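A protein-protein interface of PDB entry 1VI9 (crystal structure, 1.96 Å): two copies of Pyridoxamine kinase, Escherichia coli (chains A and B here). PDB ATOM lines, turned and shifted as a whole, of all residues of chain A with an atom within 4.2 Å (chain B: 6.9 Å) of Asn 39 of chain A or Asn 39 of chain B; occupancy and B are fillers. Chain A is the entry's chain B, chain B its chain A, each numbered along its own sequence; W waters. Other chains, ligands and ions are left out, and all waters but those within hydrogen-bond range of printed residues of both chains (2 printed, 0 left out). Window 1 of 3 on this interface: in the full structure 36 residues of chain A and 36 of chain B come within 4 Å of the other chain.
His 13 of chain A touches Pro 37 of chain B, and with the chains exchanged Pro 37 of chain A touches His 13 of chain B.
His 13 of chain A touches Asn 39 of chain B, and with the chains exchanged Asn 39 of chain A touches His 13 of chain B.
Pro 37 of chain A touches Gln 42 of chain B, but with the chains exchanged Gln 42 of chain A does not touch Pro 37 of chain B (4.2 Å).
Leu 38 of chain A touches Gln 42 of chain B, but with the chains exchanged Gln 42 of chain A does not touch Leu 38 of chain B (4.1 Å).
Printed residues of chain B that touch a printed residue of chain A: His 13, Val 15, Pro 37, Asn 39, Gln 42, Met 57, His 61 and Ile 65.
Along chain A the printed residues that touch a printed residue of chain B span positions 13 to 57.
Among the printed residues, 15 pairs touch across the chains.
O of Pro 37 of chain A is in hydrogen-bond range of NE2 of His 13 of chain B.
NE2 of His 13 of chain A is in hydrogen-bond range of O of Pro 37 of chain B, at 2.8 Å.
The backbone carbonyl oxygen of Asn 39 of chain A sits at hydrogen-bond distance from the side-chain amide nitrogen of Gln 42 of chain B (3.0 Å).
The backbone carbonyl oxygen (O) of Asn 39 of chain B is in hydrogen-bond range of the side-chain amide nitrogen (NE2) of Gln 42 of chain A (2.9 Å).
A ring nitrogen (NE2) of His 61 of chain B is in hydrogen-bond range of the side-chain amide nitrogen (NE2) of Gln 42 of chain A (3.0 Å).
Of the printed residues of chain B, His 13 of chain A touches Pro 37 (2.8 Å) and Asn 39 (3.8 Å).
Printed residues of chain B within 4 Å of Leu 38 of chain A: Val 15 (3.9 Å) and Gln 42 (3.9 Å).
Of chain B, only His 13, Asn 39 and Gln 42 come within 4 Å of Asn 39 of chain A.
Of the printed residues of chain A, His 13 of chain B touches Pro 37 (2.7 Å) and Asn 39 (3.7 Å).
Printed residues of chain A within 4 Å of Ile 65 of chain B: Gln 42 (3.7 Å).
The nearest printed residue of chain A that does not touch Gln 42 of chain B is Thr 40 of chain A (5.1 Å).
Water W1 lies within hydrogen-bond range of the side-chain amide oxygen (OE1) of Gln 42 of chain A (2.4 Å), the side-chain amide nitrogen (ND2) of Asn 39 of chain A (3.0 Å) and the side-chain amide nitrogen (ND2) of Asn 39 of chain B (3.1 Å).
Water W2 lies within hydrogen-bond range of ND2 of Asn 39 of chain B (2.8 Å), ND1 of His 13 of chain B (3.2 Å) and ND2 of Asn 39 of chain A (3.5 Å).
The side-chain amide oxygen (OD1) of Asn 39 of chain B sits at hydrogen-bond distance from the side-chain amide nitrogen (ND2) of Asn 21 of chain B (3.0 Å).
N of His 13 of chain A lies within hydrogen-bond range of O of Val 41 of chain A (3.1 Å).
OD1 of Asn 39 of chain A is in hydrogen-bond range of ND2 of Asn 21 of chain A.
The backbone carbonyl oxygen of Leu 38 of chain A sits at hydrogen-bond distance from the backbone NH of Gln 11 of chain A, 3.4 Å away.
O of Thr 40 of chain A is in hydrogen-bond range of N of Met 57 of chain A, at 2.9 Å.
NE2 of His 13 of chain B lies close to OE1 of Gln 42 of chain B, 3.3 Å away.
ND2 of Asn 39 of chain B touches NE2 of His 13 of chain A, 3.8 Å away.
Val 15 of chain B touches Pro 37 of chain A.
Gln 42 of chain B touches Pro 37 of chain A (OE1 to O, 3.6 Å).
CB of Leu 38 of chain A touches CG1 of Val 15 of chain B, 3.9 Å away.
NE2 of Gln 42 of chain B touches CD1 of Leu 38 of chain A (3.9 Å).
ND2 of Asn 39 of chain A touches NE2 of His 13 of chain B (3.7 Å).
ND2 of Asn 39 of chain B touches ND2 of Asn 39 of chain A, 3.8 Å away.
Gln 42 of chain A touches Met 57 of chain B (NE2 to CE, 3.2 Å).
O of Gln 42 of chain A touches CD1 of Ile 65 of chain B, 3.7 Å away.
Met 57 of chain A touches Gln 42 of chain B (CE to NE2, 3.6 Å).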
ATOM      1  N   GLN A  11      17.198  -8.051  29.985  1.00  0.00           N
ATOM      2  CA  GLN A  11      18.545  -8.177  29.450  1.00  0.00           C
ATOM      3  C   GLN A  11      19.180  -6.828  29.227  1.00  0.00           C
ATOM      4  O   GLN A  11      18.573  -5.808  29.597  1.00  0.00           O
ATOM      5  CB  GLN A  11      18.598  -9.048  28.188  1.00  0.00           C
ATOM      6  CG  GLN A  11      17.634  -8.621  27.093  1.00  0.00           C
ATOM      7  CD  GLN A  11      17.601  -9.644  25.961  1.00  0.00           C
ATOM      8  OE1 GLN A  11      18.540 -10.426  25.799  1.00  0.00           O
ATOM      9  NE2 GLN A  11      16.547  -9.618  25.159  1.00  0.00           N
ATOM     10  N   HIS A  13      21.096  -3.248  27.820  1.00  0.00           N
ATOM     11  CA  HIS A  13      20.720  -2.184  26.881  1.00  0.00           C
ATOM     12  C   HIS A  13      21.968  -1.384  26.522  1.00  0.00           C
ATOM     13  O   HIS A  13      22.715  -0.967  27.410  1.00  0.00           O
ATOM     14  CB  HIS A  13      19.637  -1.269  27.380  1.00  0.00           C
ATOM     15  CG  HIS A  13      19.399  -0.054  26.541  1.00  0.00           C
ATOM     16  ND1 HIS A  13      18.825  -0.143  25.306  1.00  0.00           N
ATOM     17  CD2 HIS A  13      19.624   1.263  26.753  1.00  0.00           C
ATOM     18  CE1 HIS A  13      18.706   1.066  24.786  1.00  0.00           C
ATOM     19  NE2 HIS A  13      19.205   1.948  25.642  1.00  0.00           N
ATOM     20  N   ASN A  21      18.658  -6.366  24.781  1.00  0.00           N
ATOM     21  CA  ASN A  21      17.360  -5.841  24.374  1.00  0.00           C
ATOM     22  C   ASN A  21      17.520  -4.894  23.182  1.00  0.00           C
ATOM     23  O   ASN A  21      16.620  -4.789  22.340  1.00  0.00           O
ATOM     24  CB  ASN A  21      16.667  -5.091  25.522  1.00  0.00           C
ATOM     25  CG  ASN A  21      15.799  -5.935  26.396  1.00  0.00           C
ATOM     26  OD1 ASN A  21      15.320  -6.998  25.967  1.00  0.00           O
ATOM     27  ND2 ASN A  21      15.625  -5.536  27.674  1.00  0.00           N
ATOM     28  N   PRO A  37      10.753  -3.916  27.869  1.00  0.00           N
ATOM     29  CA  PRO A  37      12.185  -3.975  28.017  1.00  0.00           C
ATOM     30  C   PRO A  37      12.750  -3.517  29.348  1.00  0.00           C
ATOM     31  O   PRO A  37      12.795  -2.337  29.627  1.00  0.00           O
ATOM     32  CB  PRO A  37      12.725  -3.175  26.859  1.00  0.00           C
ATOM     33  CG  PRO A  37      11.556  -2.563  26.173  1.00  0.00           C
ATOM     34  CD  PRO A  37      10.356  -2.708  27.108  1.00  0.00           C
ATOM     35  N   LEU A  38      12.960  -4.503  30.232  1.00  0.00           N
ATOM     36  CA  LEU A  38      13.504  -4.221  31.556  1.00  0.00           C
ATOM     37  C   LEU A  38      15.018  -4.417  31.418  1.00  0.00           C
ATOM     38  O   LEU A  38      15.520  -5.544  31.495  1.00  0.00           O
ATOM     39  CB  LEU A  38      12.897  -5.135  32.604  1.00  0.00           C
ATOM     40  CG  LEU A  38      13.466  -5.096  34.023  1.00  0.00           C
ATOM     41  CD1 LEU A  38      13.629  -3.692  34.562  1.00  0.00           C
ATOM     42  CD2 LEU A  38      12.552  -5.927  34.940  1.00  0.00           C
ATOM     43  N   ASN A  39      15.703  -3.314  31.157  1.00  0.00           N
ATOM     44  CA  ASN A  39      17.128  -3.319  30.937  1.00  0.00           C
ATOM     45  C   ASN A  39      17.938  -3.583  32.203  1.00  0.00           C
ATOM     46  O   ASN A  39      17.750  -3.000  33.268  1.00  0.00           O
ATOM     47  CB  ASN A  39      17.548  -2.058  30.200  1.00  0.00           C
ATOM     48  CG  ASN A  39      16.704  -1.776  28.954  1.00  0.00           C
ATOM     49  OD1 ASN A  39      16.398  -2.678  28.196  1.00  0.00           O
ATOM     50  ND2 ASN A  39      16.418  -0.498  28.696  1.00  0.00           N
ATOM     51  N   THR A  40      18.869  -4.526  32.090  1.00  0.00           N
ATOM     52  CA  THR A  40      19.709  -4.906  33.227  1.00  0.00           C
ATOM     53  C   THR A  40      20.881  -3.981  33.393  1.00  0.00           C
ATOM     54  O   THR A  40      21.463  -3.826  34.489  1.00  0.00           O
ATOM     55  CB  THR A  40      20.153  -6.373  33.065  1.00  0.00           C
ATOM     56  OG1 THR A  40      20.808  -6.434  31.798  1.00  0.00           O
ATOM     57  CG2 THR A  40      18.921  -7.277  33.087  1.00  0.00           C
ATOM     58  N   VAL A  41      21.301  -3.340  32.305  1.00  0.00           N
ATOM     59  CA  VAL A  41      22.368  -2.393  32.279  1.00  0.00           C
ATOM     60  C   VAL A  41      22.031  -1.316  31.211  1.00  0.00           C
ATOM     61  O   VAL A  41      21.143  -1.579  30.403  1.00  0.00           O
ATOM     62  CB  VAL A  41      23.728  -2.961  31.789  1.00  0.00           C
ATOM     63  CG1 VAL A  41      24.275  -4.060  32.690  1.00  0.00           C
ATOM     64  CG2 VAL A  41      23.589  -3.469  30.356  1.00  0.00           C
ATOM     65  N   GLN A  42      22.597  -0.136  31.384  1.00  0.00           N
ATOM     66  CA  GLN A  42      22.622   0.853  30.314  1.00  0.00           C
ATOM     67  C   GLN A  42      24.050   1.299  30.015  1.00  0.00           C
ATOM     68  O   GLN A  42      24.699   2.048  30.699  1.00  0.00           O
ATOM     69  CB  GLN A  42      21.501   1.874  30.509  1.00  0.00           C
ATOM     70  CG  GLN A  42      21.691   3.163  29.724  1.00  0.00           C
ATOM     71  CD  GLN A  42      20.422   3.990  29.644  1.00  0.00           C
ATOM     72  OE1 GLN A  42      19.426   3.565  29.060  1.00  0.00           O
ATOM     73  NE2 GLN A  42      20.455   5.179  30.234  1.00  0.00           N
ATOM     74  N   MET A  57      22.050  -1.858  36.489  1.00  0.00           N
ATOM     75  CA  MET A  57      20.884  -1.506  37.324  1.00  0.00           C
ATOM     76  C   MET A  57      20.928  -2.379  38.567  1.00  0.00           C
ATOM     77  O   MET A  57      21.303  -3.552  38.506  1.00  0.00           O
ATOM     78  CB  MET A  57      19.620  -1.722  36.520  1.00  0.00           C
ATOM     79  CG  MET A  57      19.632  -1.034  35.153  1.00  0.00           C
ATOM     80  SD  MET A  57      19.768   0.857  35.264  1.00  0.00           S
ATOM     81  CE  MET A  57      18.046   1.338  35.872  1.00  0.00           C
ATOM     82  N   LEU A  62      15.149  -4.118  39.522  1.00  0.00           N
ATOM     83  CA  LEU A  62      14.427  -5.077  38.660  1.00  0.00           C
ATOM     84  C   LEU A  62      13.140  -5.511  39.347  1.00  0.00           C
ATOM     85  O   LEU A  62      12.067  -5.485  38.745  1.00  0.00           O
ATOM     86  CB  LEU A  62      15.304  -6.278  38.353  1.00  0.00           C
ATOM     87  CG  LEU A  62      16.673  -5.991  37.725  1.00  0.00           C
ATOM     88  CD1 LEU A  62      17.328  -7.302  37.338  1.00  0.00           C
ATOM     89  CD2 LEU A  62      16.490  -5.079  36.508  1.00  0.00           C
ATOM     90  N   ALA B   9      18.336   9.846  20.835  1.00  0.00           N
ATOM     91  CA  ALA B   9      17.109  10.292  21.519  1.00  0.00           C
ATOM     92  C   ALA B   9      17.272  10.164  23.015  1.00  0.00           C
ATOM     93  O   ALA B   9      17.552   9.077  23.533  1.00  0.00           O
ATOM     94  CB  ALA B   9      15.960   9.428  20.986  1.00  0.00           C
ATOM     95  N   ILE B  10      17.214  11.287  23.721  1.00  0.00           N
ATOM     96  CA  ILE B  10      17.424  11.413  25.147  1.00  0.00           C
ATOM     97  C   ILE B  10      16.140  11.802  25.854  1.00  0.00           C
ATOM     98  O   ILE B  10      15.674  12.961  25.818  1.00  0.00           O
ATOM     99  CB  ILE B  10      18.526  12.485  25.442  1.00  0.00           C
ATOM    100  CG1 ILE B  10      19.702  12.277  24.461  1.00  0.00           C
ATOM    101  CG2 ILE B  10      19.012  12.296  26.874  1.00  0.00           C
ATOM    102  CD1 ILE B  10      20.746  13.384  24.503  1.00  0.00           C
ATOM    103  N   GLN B  11      15.388  10.746  26.203  1.00  0.00           N
ATOM    104  CA  GLN B  11      14.078  10.827  26.799  1.00  0.00           C
ATOM    105  C   GLN B  11      13.836   9.615  27.705  1.00  0.00           C
ATOM    106  O   GLN B  11      14.651   8.712  27.748  1.00  0.00           O
ATOM    107  CB  GLN B  11      12.935  10.794  25.760  1.00  0.00           C
ATOM    108  CG  GLN B  11      13.116  11.740  24.603  1.00  0.00           C
ATOM    109  CD  GLN B  11      12.005  11.675  23.588  1.00  0.00           C
ATOM    110  OE1 GLN B  11      11.093  12.503  23.703  1.00  0.00           O
ATOM    111  NE2 GLN B  11      12.119  10.739  22.658  1.00  0.00           N
ATOM    112  N   SER B  12      12.692   9.612  28.366  1.00  0.00           N
ATOM    113  CA  SER B  12      12.332   8.575  29.301  1.00  0.00           C
ATOM    114  C   SER B  12      12.075   7.201  28.666  1.00  0.00           C
ATOM    115  O   SER B  12      11.756   7.135  27.492  1.00  0.00           O
ATOM    116  CB  SER B  12      11.026   8.954  30.035  1.00  0.00           C
ATOM    117  OG  SER B  12      11.265  10.087  30.837  1.00  0.00           O
ATOM    118  N   HIS B  13      12.203   6.190  29.521  1.00  0.00           N
ATOM    119  CA  HIS B  13      11.927   4.808  29.147  1.00  0.00           C
ATOM    120  C   HIS B  13      11.011   4.199  30.218  1.00  0.00           C
ATOM    121  O   HIS B  13      11.169   4.447  31.419  1.00  0.00           O
ATOM    122  CB  HIS B  13      13.158   3.953  28.942  1.00  0.00           C
ATOM    123  CG  HIS B  13      12.990   2.468  28.877  1.00  0.00           C
ATOM    124  ND1 HIS B  13      12.611   1.782  27.751  1.00  0.00           N
ATOM    125  CD2 HIS B  13      13.123   1.531  29.844  1.00  0.00           C
ATOM    126  CE1 HIS B  13      12.542   0.500  27.995  1.00  0.00           C
ATOM    127  NE2 HIS B  13      12.849   0.309  29.258  1.00  0.00           N
ATOM    128  N   VAL B  14       9.971   3.534  29.752  1.00  0.00           N
ATOM    129  CA  VAL B  14       8.981   2.862  30.573  1.00  0.00           C
ATOM    130  C   VAL B  14       8.983   1.383  30.152  1.00  0.00           C
ATOM    131  O   VAL B  14       9.011   1.073  28.939  1.00  0.00           O
ATOM    132  CB  VAL B  14       7.593   3.482  30.501  1.00  0.00           C
ATOM    133  CG1 VAL B  14       7.537   4.849  31.202  1.00  0.00           C
ATOM    134  CG2 VAL B  14       7.101   3.708  29.044  1.00  0.00           C
ATOM    135  N   VAL B  15       9.040   0.506  31.143  1.00  0.00           N
ATOM    136  CA  VAL B  15       9.100  -0.934  30.872  1.00  0.00           C
ATOM    137  C   VAL B  15       7.811  -1.411  30.262  1.00  0.00           C
ATOM    138  O   VAL B  15       7.807  -2.074  29.229  1.00  0.00           O
ATOM    139  CB  VAL B  15       9.547  -1.743  32.086  1.00  0.00           C
ATOM    140  CG1 VAL B  15       9.598  -3.226  31.761  1.00  0.00           C
ATOM    141  CG2 VAL B  15      10.927  -1.235  32.500  1.00  0.00           C
ATOM    142  N   ASN B  21      11.042   7.892  25.002  1.00  0.00           N
ATOM    143  CA  ASN B  21      11.740   7.024  24.045  1.00  0.00           C
ATOM    144  C   ASN B  21      10.960   5.745  23.780  1.00  0.00           C
ATOM    145  O   ASN B  21      11.046   5.178  22.699  1.00  0.00           O
ATOM    146  CB  ASN B  21      13.134   6.723  24.572  1.00  0.00           C
ATOM    147  CG  ASN B  21      14.210   7.706  24.160  1.00  0.00           C
ATOM    148  OD1 ASN B  21      14.000   8.524  23.267  1.00  0.00           O
ATOM    149  ND2 ASN B  21      15.376   7.505  24.785  1.00  0.00           N
ATOM    150  N   SER B  22      10.231   5.245  24.790  1.00  0.00           N
ATOM    151  CA  SER B  22       9.418   4.054  24.655  1.00  0.00           C
ATOM    152  C   SER B  22       8.227   4.252  23.702  1.00  0.00           C
ATOM    153  O   SER B  22       7.615   3.252  23.253  1.00  0.00           O
ATOM    154  CB  SER B  22       8.946   3.579  26.011  1.00  0.00           C
ATOM    155  OG  SER B  22      10.054   3.355  26.876  1.00  0.00           O
ATOM    156  N   TRP B  36      19.369   5.733  18.803  1.00  0.00           N
ATOM    157  CA  TRP B  36      20.307   5.388  19.910  1.00  0.00           C
ATOM    158  C   TRP B  36      19.586   5.879  21.170  1.00  0.00           C
ATOM    159  O   TRP B  36      19.479   7.088  21.382  1.00  0.00           O
ATOM    160  CB  TRP B  36      21.627   6.134  19.780  1.00  0.00           C
ATOM    161  CG  TRP B  36      22.371   5.958  18.479  1.00  0.00           C
ATOM    162  CD1 TRP B  36      22.157   5.081  17.474  1.00  0.00           C
ATOM    163  CD2 TRP B  36      23.521   6.721  18.102  1.00  0.00           C
ATOM    164  NE1 TRP B  36      23.104   5.236  16.470  1.00  0.00           N
ATOM    165  CE2 TRP B  36      23.951   6.237  16.834  1.00  0.00           C
ATOM    166  CE3 TRP B  36      24.288   7.695  18.749  1.00  0.00           C
ATOM    167  CZ2 TRP B  36      25.061   6.742  16.150  1.00  0.00           C
ATOM    168  CZ3 TRP B  36      25.398   8.207  18.066  1.00  0.00           C
ATOM    169  CH2 TRP B  36      25.765   7.729  16.813  1.00  0.00           C
ATOM    170  N   PRO B  37      18.893   4.999  21.861  1.00  0.00           N
ATOM    171  CA  PRO B  37      18.046   5.422  22.983  1.00  0.00           C
ATOM    172  C   PRO B  37      18.787   5.600  24.293  1.00  0.00           C
ATOM    173  O   PRO B  37      19.062   4.618  24.996  1.00  0.00           O
ATOM    174  CB  PRO B  37      16.987   4.310  23.075  1.00  0.00           C
ATOM    175  CG  PRO B  37      17.279   3.376  21.935  1.00  0.00           C
ATOM    176  CD  PRO B  37      18.796   3.551  21.702  1.00  0.00           C
ATOM    177  N   LEU B  38      19.064   6.851  24.602  1.00  0.00           N
ATOM    178  CA  LEU B  38      19.756   7.259  25.808  1.00  0.00           C
ATOM    179  C   LEU B  38      18.656   7.618  26.828  1.00  0.00           C
ATOM    180  O   LEU B  38      18.270   8.765  26.962  1.00  0.00           O
ATOM    181  CB  LEU B  38      20.607   8.496  25.537  1.00  0.00           C
ATOM    182  CG  LEU B  38      21.832   8.724  26.403  1.00  0.00           C
ATOM    183  CD1 LEU B  38      22.352  10.145  26.257  1.00  0.00           C
ATOM    184  CD2 LEU B  38      21.656   8.308  27.838  1.00  0.00           C
ATOM    185  N   ASN B  39      18.164   6.582  27.475  1.00  0.00           N
ATOM    186  CA  ASN B  39      17.091   6.662  28.416  1.00  0.00           C
ATOM    187  C   ASN B  39      17.459   7.457  29.667  1.00  0.00           C
ATOM    188  O   ASN B  39      18.413   7.202  30.374  1.00  0.00           O
ATOM    189  CB  ASN B  39      16.591   5.272  28.776  1.00  0.00           C
ATOM    190  CG  ASN B  39      16.156   4.493  27.531  1.00  0.00           C
ATOM    191  OD1 ASN B  39      15.744   5.022  26.505  1.00  0.00           O
ATOM    192  ND2 ASN B  39      16.204   3.186  27.621  1.00  0.00           N
ATOM    193  N   THR B  40      16.608   8.442  29.940  1.00  0.00           N
ATOM    194  CA  THR B  40      16.842   9.318  31.099  1.00  0.00           C
ATOM    195  C   THR B  40      16.347   8.741  32.397  1.00  0.00           C
ATOM    196  O   THR B  40      16.713   9.221  33.490  1.00  0.00           O
ATOM    197  CB  THR B  40      16.178  10.668  30.797  1.00  0.00           C
ATOM    198  OG1 THR B  40      14.779  10.456  30.602  1.00  0.00           O
ATOM    199  CG2 THR B  40      16.782  11.239  29.509  1.00  0.00           C
ATOM    200  N   VAL B  41      15.506   7.722  32.350  1.00  0.00           N
ATOM    201  CA  VAL B  41      14.914   7.036  33.468  1.00  0.00           C
ATOM    202  C   VAL B  41      14.535   5.602  33.017  1.00  0.00           C
ATOM    203  O   VAL B  41      14.556   5.271  31.850  1.00  0.00           O
ATOM    204  CB  VAL B  41      13.601   7.639  33.999  1.00  0.00           C
ATOM    205  CG1 VAL B  41      13.630   9.162  34.226  1.00  0.00           C
ATOM    206  CG2 VAL B  41      12.423   7.345  33.060  1.00  0.00           C
ATOM    207  N   GLN B  42      14.316   4.746  33.966  1.00  0.00           N
ATOM    208  CA  GLN B  42      13.627   3.477  33.769  1.00  0.00           C
ATOM    209  C   GLN B  42      12.588   3.245  34.862  1.00  0.00           C
ATOM    210  O   GLN B  42      12.889   3.137  36.030  1.00  0.00           O
ATOM    211  CB  GLN B  42      14.627   2.385  33.386  1.00  0.00           C
ATOM    212  CG  GLN B  42      14.113   0.970  33.600  1.00  0.00           C
ATOM    213  CD  GLN B  42      14.997  -0.077  32.951  1.00  0.00           C
ATOM    214  OE1 GLN B  42      14.879  -0.349  31.755  1.00  0.00           O
ATOM    215  NE2 GLN B  42      15.889  -0.668  33.735  1.00  0.00           N
ATOM    216  N   MET B  57      17.942   8.479  35.946  1.00  0.00           N
ATOM    217  CA  MET B  57      19.398   8.444  35.707  1.00  0.00           C
ATOM    218  C   MET B  57      19.919   9.862  35.974  1.00  0.00           C
ATOM    219  O   MET B  57      19.271  10.807  35.548  1.00  0.00           O
ATOM    220  CB  MET B  57      19.705   8.086  34.251  1.00  0.00           C
ATOM    221  CG  MET B  57      19.066   6.791  33.764  1.00  0.00           C
ATOM    222  SD  MET B  57      19.806   5.283  34.681  1.00  0.00           S
ATOM    223  CE  MET B  57      20.853   4.480  33.323  1.00  0.00           C
ATOM    224  N   HIS B  61      25.120  10.822  33.984  1.00  0.00           N
ATOM    225  CA  HIS B  61      25.089   9.553  33.254  1.00  0.00           C
ATOM    226  C   HIS B  61      24.892   9.784  31.758  1.00  0.00           C
ATOM    227  O   HIS B  61      25.511   9.101  30.943  1.00  0.00           O
ATOM    228  CB  HIS B  61      23.989   8.636  33.799  1.00  0.00           C
ATOM    229  CG  HIS B  61      23.742   7.400  32.980  1.00  0.00           C
ATOM    230  ND1 HIS B  61      24.506   6.277  33.052  1.00  0.00           N
ATOM    231  CD2 HIS B  61      22.793   7.172  32.021  1.00  0.00           C
ATOM    232  CE1 HIS B  61      24.052   5.357  32.200  1.00  0.00           C
ATOM    233  NE2 HIS B  61      22.999   5.894  31.567  1.00  0.00           N
ATOM    234  N   LEU B  62      24.063  10.756  31.375  1.00  0.00           N
ATOM    235  CA  LEU B  62      23.856  11.043  29.955  1.00  0.00           C
ATOM    236  C   LEU B  62      25.186  11.405  29.289  1.00  0.00           C
ATOM    237  O   LEU B  62      25.621  10.844  28.284  1.00  0.00           O
ATOM    238  CB  LEU B  62      22.857  12.200  29.784  1.00  0.00           C
ATOM    239  CG  LEU B  62      21.613  12.178  30.661  1.00  0.00           C
ATOM    240  CD1 LEU B  62      20.684  13.336  30.371  1.00  0.00           C
ATOM    241  CD2 LEU B  62      20.866  10.850  30.588  1.00  0.00           C
ATOM    242  N   ILE B  65      27.567   8.442  28.969  1.00  0.00           N
ATOM    243  CA  ILE B  65      27.186   7.585  27.845  1.00  0.00           C
ATOM    244  C   ILE B  65      27.757   8.178  26.558  1.00  0.00           C
ATOM    245  O   ILE B  65      28.410   7.535  25.740  1.00  0.00           O
ATOM    246  CB  ILE B  65      25.653   7.514  27.725  1.00  0.00           C
ATOM    247  CG1 ILE B  65      25.040   6.724  28.859  1.00  0.00           C
ATOM    248  CG2 ILE B  65      25.251   6.916  26.352  1.00  0.00           C
ATOM    249  CD1 ILE B  65      25.430   5.233  28.905  1.00  0.00           C
HETATM  250  O   HOH W   1      17.898   1.866  29.878  1.00  0.00           O
HETATM  251  O   HOH W   2      15.143   1.168  25.949  1.00  0.00           O
